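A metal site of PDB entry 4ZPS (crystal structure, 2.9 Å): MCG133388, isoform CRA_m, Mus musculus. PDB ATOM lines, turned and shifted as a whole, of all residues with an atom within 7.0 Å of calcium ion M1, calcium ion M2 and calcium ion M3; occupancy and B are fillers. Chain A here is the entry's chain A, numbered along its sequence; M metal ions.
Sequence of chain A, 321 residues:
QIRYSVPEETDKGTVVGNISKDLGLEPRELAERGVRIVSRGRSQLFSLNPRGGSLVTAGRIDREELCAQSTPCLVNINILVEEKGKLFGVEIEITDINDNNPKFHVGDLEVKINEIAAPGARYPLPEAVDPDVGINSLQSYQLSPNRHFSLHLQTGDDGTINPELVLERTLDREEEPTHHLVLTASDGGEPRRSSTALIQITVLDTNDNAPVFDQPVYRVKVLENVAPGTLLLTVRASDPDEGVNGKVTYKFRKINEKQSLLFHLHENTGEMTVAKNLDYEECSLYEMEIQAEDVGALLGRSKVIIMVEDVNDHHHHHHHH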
ATOM      1  N   ASN A 114       1.962  -2.952 -13.194  1.00  0.00           N
ATOM      2  CA  ASN A 114       2.566  -2.170 -12.124  1.00  0.00           C
ATOM      3  C   ASN A 114       4.053  -1.965 -12.362  1.00  0.00           C
ATOM      4  O   ASN A 114       4.708  -2.794 -12.980  1.00  0.00           O
ATOM      5  CB  ASN A 114       2.326  -2.859 -10.774  1.00  0.00           C
ATOM      6  CG  ASN A 114       2.620  -1.957  -9.591  1.00  0.00           C
ATOM      7  OD1 ASN A 114       3.582  -1.193  -9.590  1.00  0.00           O
ATOM      8  ND2 ASN A 114       1.771  -2.032  -8.574  1.00  0.00           N
ATOM      9  N   GLU A 115       4.585  -0.844 -11.864  1.00  0.00           N
ATOM     10  CA  GLU A 115       6.002  -0.533 -12.000  1.00  0.00           C
ATOM     11  C   GLU A 115       6.895  -1.581 -11.357  1.00  0.00           C
ATOM     12  O   GLU A 115       8.005  -1.830 -11.829  1.00  0.00           O
ATOM     13  CB  GLU A 115       6.318   0.825 -11.365  1.00  0.00           C
ATOM     14  CG  GLU A 115       5.738   2.032 -12.051  1.00  0.00           C
ATOM     15  CD  GLU A 115       6.092   3.291 -11.317  1.00  0.00           C
ATOM     16  OE1 GLU A 115       6.136   3.261 -10.071  1.00  0.00           O
ATOM     17  OE2 GLU A 115       6.339   4.324 -11.982  1.00  0.00           O
ATOM     18  N   LEU A 171       9.253  -0.696 -16.084  1.00  0.00           N
ATOM     19  CA  LEU A 171       8.438   0.483 -16.376  1.00  0.00           C
ATOM     20  C   LEU A 171       8.571   1.523 -15.253  1.00  0.00           C
ATOM     21  O   LEU A 171       9.104   1.228 -14.180  1.00  0.00           O
ATOM     22  CB  LEU A 171       6.968   0.095 -16.567  1.00  0.00           C
ATOM     23  CG  LEU A 171       6.671  -0.785 -17.789  1.00  0.00           C
ATOM     24  CD1 LEU A 171       5.231  -1.276 -17.767  1.00  0.00           C
ATOM     25  CD2 LEU A 171       6.944  -0.027 -19.074  1.00  0.00           C
ATOM     26  N   ASP A 172       8.083   2.732 -15.524  1.00  0.00           N
ATOM     27  CA  ASP A 172       8.136   3.821 -14.554  1.00  0.00           C
ATOM     28  C   ASP A 172       7.127   4.903 -14.924  1.00  0.00           C
ATOM     29  O   ASP A 172       7.378   5.714 -15.817  1.00  0.00           O
ATOM     30  CB  ASP A 172       9.545   4.403 -14.470  1.00  0.00           C
ATOM     31  CG  ASP A 172       9.661   5.516 -13.438  1.00  0.00           C
ATOM     32  OD1 ASP A 172       8.875   5.518 -12.467  1.00  0.00           O
ATOM     33  OD2 ASP A 172      10.549   6.380 -13.604  1.00  0.00           O
ATOM     34  N   ARG A 173       5.980   4.930 -14.237  1.00  0.00           N
ATOM     35  CA  ARG A 173       4.931   5.895 -14.556  1.00  0.00           C
ATOM     36  C   ARG A 173       5.301   7.304 -14.102  1.00  0.00           C
ATOM     37  O   ARG A 173       4.664   8.282 -14.483  1.00  0.00           O
ATOM     38  CB  ARG A 173       3.591   5.480 -13.944  1.00  0.00           C
ATOM     39  CG  ARG A 173       3.528   5.586 -12.435  1.00  0.00           C
ATOM     40  CD  ARG A 173       2.131   5.964 -11.958  1.00  0.00           C
ATOM     41  NE  ARG A 173       1.781   7.331 -12.342  1.00  0.00           N
ATOM     42  CZ  ARG A 173       2.135   8.413 -11.654  1.00  0.00           C
ATOM     43  NH1 ARG A 173       2.856   8.287 -10.553  1.00  0.00           N
ATOM     44  NH2 ARG A 173       1.775   9.614 -12.079  1.00  0.00           N
ATOM     45  N   GLU A 174       6.330   7.403 -13.269  1.00  0.00           N
ATOM     46  CA  GLU A 174       6.844   8.710 -12.867  1.00  0.00           C
ATOM     47  C   GLU A 174       7.516   9.385 -14.058  1.00  0.00           C
ATOM     48  O   GLU A 174       7.701  10.606 -14.072  1.00  0.00           O
ATOM     49  CB  GLU A 174       7.822   8.586 -11.692  1.00  0.00           C
ATOM     50  CG  GLU A 174       7.141   8.514 -10.333  1.00  0.00           C
ATOM     51  CD  GLU A 174       6.438   7.192 -10.077  1.00  0.00           C
ATOM     52  OE1 GLU A 174       5.194   7.162 -10.095  1.00  0.00           O
ATOM     53  OE2 GLU A 174       7.140   6.181  -9.848  1.00  0.00           O
ATOM     54  N   GLU A 175       7.860   8.585 -15.058  1.00  0.00           N
ATOM     55  CA  GLU A 175       8.403   9.095 -16.316  1.00  0.00           C
ATOM     56  C   GLU A 175       7.368   9.021 -17.435  1.00  0.00           C
ATOM     57  O   GLU A 175       7.132  10.003 -18.142  1.00  0.00           O
ATOM     58  CB  GLU A 175       9.667   8.317 -16.717  1.00  0.00           C
ATOM     59  CG  GLU A 175      10.916   8.739 -15.976  1.00  0.00           C
ATOM     60  CD  GLU A 175      11.422  10.112 -16.411  1.00  0.00           C
ATOM     61  OE1 GLU A 175      10.974  10.601 -17.467  1.00  0.00           O
ATOM     62  OE2 GLU A 175      12.268  10.685 -15.701  1.00  0.00           O
ATOM     63  N   LEU A 204       0.359   1.086 -13.769  1.00  0.00           N
ATOM     64  CA  LEU A 204      -0.164   1.353 -12.438  1.00  0.00           C
ATOM     65  C   LEU A 204       0.961   1.818 -11.524  1.00  0.00           C
ATOM     66  O   LEU A 204       2.133   1.587 -11.805  1.00  0.00           O
ATOM     67  CB  LEU A 204      -0.853   0.122 -11.861  1.00  0.00           C
ATOM     68  CG  LEU A 204      -1.962  -0.471 -12.728  1.00  0.00           C
ATOM     69  CD1 LEU A 204      -2.685  -1.606 -12.004  1.00  0.00           C
ATOM     70  CD2 LEU A 204      -2.946   0.596 -13.166  1.00  0.00           C
ATOM     71  N   ASP A 205       0.602   2.483 -10.428  1.00  0.00           N
ATOM     72  CA  ASP A 205       1.600   3.085  -9.551  1.00  0.00           C
ATOM     73  C   ASP A 205       2.000   2.187  -8.392  1.00  0.00           C
ATOM     74  O   ASP A 205       1.192   1.391  -7.897  1.00  0.00           O
ATOM     75  CB  ASP A 205       1.075   4.415  -8.998  1.00  0.00           C
ATOM     76  CG  ASP A 205       2.136   5.183  -8.219  1.00  0.00           C
ATOM     77  OD1 ASP A 205       2.924   5.930  -8.836  1.00  0.00           O
ATOM     78  OD2 ASP A 205       2.178   5.044  -6.974  1.00  0.00           O
ATOM     79  N   THR A 206       3.251   2.312  -7.977  1.00  0.00           N
ATOM     80  CA  THR A 206       3.722   1.740  -6.714  1.00  0.00           C
ATOM     81  C   THR A 206       4.446   2.843  -5.947  1.00  0.00           C
ATOM     82  O   THR A 206       4.980   3.774  -6.540  1.00  0.00           O
ATOM     83  CB  THR A 206       4.659   0.537  -6.938  1.00  0.00           C
ATOM     84  OG1 THR A 206       5.051   0.001  -5.659  1.00  0.00           O
ATOM     85  CG2 THR A 206       5.903   0.955  -7.707  1.00  0.00           C
ATOM     86  N   ASN A 207       4.427   2.749  -4.625  1.00  0.00           N
ATOM     87  CA  ASN A 207       5.021   3.789  -3.780  1.00  0.00           C
ATOM     88  C   ASN A 207       6.523   3.565  -3.587  1.00  0.00           C
ATOM     89  O   ASN A 207       6.953   3.037  -2.559  1.00  0.00           O
ATOM     90  CB  ASN A 207       4.311   3.842  -2.429  1.00  0.00           C
ATOM     91  CG  ASN A 207       4.812   4.965  -1.556  1.00  0.00           C
ATOM     92  OD1 ASN A 207       4.482   6.128  -1.763  1.00  0.00           O
ATOM     93  ND2 ASN A 207       5.615   4.621  -0.557  1.00  0.00           N
ATOM     94  N   ASP A 208       7.310   3.972  -4.574  1.00  0.00           N
ATOM     95  CA  ASP A 208       8.749   3.757  -4.540  1.00  0.00           C
ATOM     96  C   ASP A 208       9.523   5.063  -4.385  1.00  0.00           C
ATOM     97  O   ASP A 208      10.722   5.054  -4.095  1.00  0.00           O
ATOM     98  CB  ASP A 208       9.206   3.022  -5.802  1.00  0.00           C
ATOM     99  CG  ASP A 208       8.741   3.689  -7.082  1.00  0.00           C
ATOM    100  OD1 ASP A 208       7.665   4.328  -7.073  1.00  0.00           O
ATOM    101  OD2 ASP A 208       9.451   3.588  -8.104  1.00  0.00           O
ATOM    102  N   ASN A 209       8.842   6.184  -4.576  1.00  0.00           N
ATOM    103  CA  ASN A 209       9.465   7.489  -4.358  1.00  0.00           C
ATOM    104  C   ASN A 209       9.242   8.016  -2.950  1.00  0.00           C
ATOM    105  O   ASN A 209       8.115   8.338  -2.570  1.00  0.00           O
ATOM    106  CB  ASN A 209       8.950   8.504  -5.386  1.00  0.00           C
ATOM    107  CG  ASN A 209       9.544   8.294  -6.756  1.00  0.00           C
ATOM    108  OD1 ASN A 209       8.853   7.836  -7.672  1.00  0.00           O
ATOM    109  ND2 ASN A 209      10.813   8.631  -6.920  1.00  0.00           N
ATOM    110  N   ALA A 210      10.313   8.088  -2.177  1.00  0.00           N
ATOM    111  CA  ALA A 210      10.264   8.657  -0.837  1.00  0.00           C
ATOM    112  C   ALA A 210      10.322  10.173  -0.914  1.00  0.00           C
ATOM    113  O   ALA A 210      10.937  10.734  -1.822  1.00  0.00           O
ATOM    114  CB  ALA A 210      11.406   8.120   0.014  1.00  0.00           C
ATOM    115  N   PRO A 211       9.663  10.860   0.032  1.00  0.00           N
ATOM    116  CA  PRO A 211       9.691  12.322   0.117  1.00  0.00           C
ATOM    117  C   PRO A 211      11.103  12.891   0.201  1.00  0.00           C
ATOM    118  O   PRO A 211      11.914  12.405   0.989  1.00  0.00           O
ATOM    119  CB  PRO A 211       8.910  12.616   1.404  1.00  0.00           C
ATOM    120  CG  PRO A 211       7.990  11.453   1.547  1.00  0.00           C
ATOM    121  CD  PRO A 211       8.760  10.266   1.034  1.00  0.00           C
ATOM    122  N   SER A 238       9.444  16.852  -2.508  1.00  0.00           N
ATOM    123  CA  SER A 238       9.011  16.288  -3.782  1.00  0.00           C
ATOM    124  C   SER A 238       8.620  14.810  -3.647  1.00  0.00           C
ATOM    125  O   SER A 238       9.277  14.041  -2.954  1.00  0.00           O
ATOM    126  CB  SER A 238      10.108  16.430  -4.827  1.00  0.00           C
ATOM    127  OG  SER A 238       9.709  15.885  -6.072  1.00  0.00           O
ATOM    128  N   ASP A 239       7.542  14.438  -4.328  1.00  0.00           N
ATOM    129  CA  ASP A 239       7.068  13.060  -4.355  1.00  0.00           C
ATOM    130  C   ASP A 239       6.219  12.836  -5.593  1.00  0.00           C
ATOM    131  O   ASP A 239       5.022  13.144  -5.590  1.00  0.00           O
ATOM    132  CB  ASP A 239       6.276  12.741  -3.084  1.00  0.00           C
ATOM    133  CG  ASP A 239       6.222  11.261  -2.788  1.00  0.00           C
ATOM    134  OD1 ASP A 239       6.189  10.455  -3.744  1.00  0.00           O
ATOM    135  OD2 ASP A 239       6.215  10.893  -1.592  1.00  0.00           O
ATOM    136  N   PRO A 240       6.818  12.300  -6.661  1.00  0.00           N
ATOM    137  CA  PRO A 240       6.188  12.154  -7.977  1.00  0.00           C
ATOM    138  C   PRO A 240       5.173  11.024  -8.042  1.00  0.00           C
ATOM    139  O   PRO A 240       4.525  10.851  -9.075  1.00  0.00           O
ATOM    140  CB  PRO A 240       7.375  11.856  -8.907  1.00  0.00           C
ATOM    141  CG  PRO A 240       8.614  12.108  -8.095  1.00  0.00           C
ATOM    142  CD  PRO A 240       8.226  11.857  -6.685  1.00  0.00           C
ATOM    143  N   ASP A 241       5.039  10.256  -6.956  1.00  0.00           N
ATOM    144  CA  ASP A 241       4.096   9.142  -6.923  1.00  0.00           C
ATOM    145  C   ASP A 241       2.658   9.623  -7.117  1.00  0.00           C
ATOM    146  O   ASP A 241       2.361  10.800  -6.951  1.00  0.00           O
ATOM    147  CB  ASP A 241       4.231   8.372  -5.610  1.00  0.00           C
ATOM    148  CG  ASP A 241       5.561   7.659  -5.492  1.00  0.00           C
ATOM    149  OD1 ASP A 241       6.189   7.393  -6.534  1.00  0.00           O
ATOM    150  OD2 ASP A 241       5.972   7.361  -4.348  1.00  0.00           O
ATOM    151  N   GLU A 242       1.777   8.693  -7.462  1.00  0.00           N
ATOM    152  CA  GLU A 242       0.415   9.036  -7.846  1.00  0.00           C
ATOM    153  C   GLU A 242      -0.521   9.190  -6.646  1.00  0.00           C
ATOM    154  O   GLU A 242      -0.578   8.321  -5.778  1.00  0.00           O
ATOM    155  CB  GLU A 242      -0.146   7.991  -8.803  1.00  0.00           C
ATOM    156  CG  GLU A 242      -1.537   8.312  -9.338  1.00  0.00           C
ATOM    157  CD  GLU A 242      -1.966   7.340 -10.432  1.00  0.00           C
ATOM    158  OE1 GLU A 242      -1.232   6.359 -10.675  1.00  0.00           O
ATOM    159  OE2 GLU A 242      -3.034   7.571 -11.041  1.00  0.00           O
ATOM    160  N   VAL A 244      -2.413   9.368  -3.528  1.00  0.00           N
ATOM    161  CA  VAL A 244      -2.201   9.125  -2.109  1.00  0.00           C
ATOM    162  C   VAL A 244      -0.726   8.884  -1.798  1.00  0.00           C
ATOM    163  O   VAL A 244      -0.214   9.306  -0.755  1.00  0.00           O
ATOM    164  CB  VAL A 244      -3.037   7.921  -1.625  1.00  0.00           C
ATOM    165  CG1 VAL A 244      -3.016   7.848  -0.110  1.00  0.00           C
ATOM    166  CG2 VAL A 244      -4.463   8.034  -2.130  1.00  0.00           C
ATOM    167  N   ASN A 245      -0.027   8.209  -2.709  1.00  0.00           N
ATOM    168  CA  ASN A 245       1.384   7.934  -2.554  1.00  0.00           C
ATOM    169  C   ASN A 245       2.246   9.189  -2.752  1.00  0.00           C
ATOM    170  O   ASN A 245       3.446   9.174  -2.486  1.00  0.00           O
ATOM    171  CB  ASN A 245       1.833   6.849  -3.528  1.00  0.00           C
ATOM    172  CG  ASN A 245       1.165   5.519  -3.275  1.00  0.00           C
ATOM    173  OD1 ASN A 245       0.967   5.111  -2.129  1.00  0.00           O
ATOM    174  ND2 ASN A 245       0.806   4.824  -4.348  1.00  0.00           N
ATOM    175  N   GLY A 246       1.614  10.257  -3.220  1.00  0.00           N
ATOM    176  CA  GLY A 246       2.325  11.502  -3.467  1.00  0.00           C
ATOM    177  C   GLY A 246       1.966  12.572  -2.458  1.00  0.00           C
ATOM    178  O   GLY A 246       2.554  13.656  -2.457  1.00  0.00           O
ATOM    179  N   LYS A 247       0.999  12.273  -1.599  1.00  0.00           N
ATOM    180  CA  LYS A 247       0.601  13.191  -0.546  1.00  0.00           C
ATOM    181  C   LYS A 247       1.690  13.292   0.512  1.00  0.00           C
ATOM    182  O   LYS A 247       1.994  12.323   1.199  1.00  0.00           O
ATOM    183  CB  LYS A 247      -0.709  12.759   0.092  1.00  0.00           C
ATOM    184  CG  LYS A 247      -1.209  13.679   1.190  1.00  0.00           C
ATOM    185  CD  LYS A 247      -2.525  13.197   1.777  1.00  0.00           C
ATOM    186  CE  LYS A 247      -2.952  14.069   2.952  1.00  0.00           C
ATOM    187  NZ  LYS A 247      -4.245  13.628   3.533  1.00  0.00           N
ATOM    188  N   ASP A 294       5.022  10.293   3.688  1.00  0.00           N
ATOM    189  CA  ASP A 294       3.912   9.864   2.836  1.00  0.00           C
ATOM    190  C   ASP A 294       3.182   8.687   3.487  1.00  0.00           C
ATOM    191  O   ASP A 294       3.593   8.199   4.538  1.00  0.00           O
ATOM    192  CB  ASP A 294       4.400   9.485   1.442  1.00  0.00           C
ATOM    193  CG  ASP A 294       5.279   8.249   1.441  1.00  0.00           C
ATOM    194  OD1 ASP A 294       5.822   7.898   2.512  1.00  0.00           O
ATOM    195  OD2 ASP A 294       5.433   7.632   0.369  1.00  0.00           O
ATOM    196  N   VAL A 295       2.111   8.222   2.848  1.00  0.00           N
ATOM    197  CA  VAL A 295       1.290   7.169   3.419  1.00  0.00           C
ATOM    198  C   VAL A 295       2.024   5.838   3.522  1.00  0.00           C
ATOM    199  O   VAL A 295       1.608   4.945   4.266  1.00  0.00           O
ATOM    200  CB  VAL A 295       0.002   6.966   2.598  1.00  0.00           C
ATOM    201  CG1 VAL A 295      -0.894   8.187   2.711  1.00  0.00           C
ATOM    202  CG2 VAL A 295       0.338   6.669   1.142  1.00  0.00           C
ATOM    203  N   GLY A 296       3.115   5.703   2.775  1.00  0.00           N
ATOM    204  CA  GLY A 296       3.916   4.501   2.837  1.00  0.00           C
ATOM    205  C   GLY A 296       4.952   4.554   3.949  1.00  0.00           C
ATOM    206  O   GLY A 296       5.823   3.695   4.034  1.00  0.00           O
ATOM    207  N   LEU A 298       7.385   6.556   4.291  1.00  0.00           N
ATOM    208  CA  LEU A 298       8.720   6.872   3.807  1.00  0.00           C
ATOM    209  C   LEU A 298       9.101   8.285   4.238  1.00  0.00           C
ATOM    210  O   LEU A 298       8.316   9.219   4.105  1.00  0.00           O
ATOM    211  CB  LEU A 298       8.805   6.741   2.288  1.00  0.00           C
ATOM    212  CG  LEU A 298       8.451   5.391   1.672  1.00  0.00           C
ATOM    213  CD1 LEU A 298       8.736   5.417   0.176  1.00  0.00           C
ATOM    214  CD2 LEU A 298       9.202   4.252   2.337  1.00  0.00           C
HETATM  215 CA    CA M   1       5.768   8.464  -2.075  1.00  0.00          CA
HETATM  216 CA    CA M   2       5.307   5.438  -8.381  1.00  0.00          CA
HETATM  217 CA    CA M   3       8.900   4.461 -10.340  1.00  0.00          CA
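The nearest printed residue that does not touch calcium ion M2 is Asn 209 (4.3 Å).
Calcium ion M1 is bound by the backbone carbonyl oxygen (O) of Asn 209 (2.4 Å). O of Asn 245 is bound to calcium ion M1. OD2 of Asp 239 is bound to calcium ion M1 (2.5 Å). The side-chain carboxylate (OD2) of Asp 241 is bound to calcium ion M1 (2.5 Å). The side-chain carboxylate (OD2) of Asp 294 binds calcium ion M1, at 2.6 Å. OD1 of Asp 239 is bound to calcium ion M1 (2.6 Å). The side-chain amide oxygen (OD1) of Asn 207 is bound to calcium ion M1 (2.7 Å). Calcium ion M1 has seven donor atoms within binding distance.
Calcium ion M3 is bound by the side-chain carboxylate of Asp 172 (2.4 Å), the side-chain carboxylate of Asp 208 (2.5 Å) and the side-chain carboxylate of Glu 174 (2.5 Å). Calcium ion M3 has three donor atoms within binding distance. Slightly farther from calcium ion M3 lies the side-chain carboxylate (OE1) of Glu 115 (3.0 Å). Slightly farther from calcium ion M3 lies OE2 of Glu 115 (3.0 Å).
OD1 of Asn 209 lies close to OE2 of Glu 174, at 3.2 Å. The side-chain carboxylate (OE1) of Glu 174 sits close to the guanidinium group (NH1) of Arg 173 (2.6 Å). The side-chain amide nitrogen of Asn 245 is in hydrogen-bond range of the side-chain carboxylate of Asp 205 (3.0 Å). OD1 of Asp 205 sits close to NH1 of Arg 173, at 2.9 Å. N of Glu 242 sits close to OD1 of Asp 205 (3.3 Å). The backbone NH (N) of Leu 298 lies within hydrogen-bond range of the side-chain carboxylate (OD1) of Asp 294 (2.7 Å). The backbone NH of Gly 296 lies close to the side-chain carboxylate of Asp 294 (3.5 Å). The backbone NH (N) of Glu 115 is in hydrogen-bond range of the backbone carbonyl oxygen (O) of Leu 204 (3.5 Å).
Calcium ion M2 is bound by the side-chain carboxylate (OE1) of Glu 174 (2.4 Å), the side-chain carboxylate (OE2) of Glu 174 (2.5 Å), the side-chain carboxylate (OD1) of Asp 205 (2.5 Å), the backbone carbonyl oxygen (O) of Thr 206 (2.5 Å), the side-chain carboxylate (OD1) of Asp 241 (2.8 Å) and the side-chain carboxylate (OE1) of Glu 115 (2.9 Å). Slightly farther from calcium ion M2 lies OD1 of Asp 208 (2.9 Å).
Four residues have an atom within 4 Å of calcium ion M3: Glu 115, Asp 172, Glu 174 and Asp 208. The nearest printed residue that does not touch calcium ion M3 is Asn 209 (4.3 Å).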
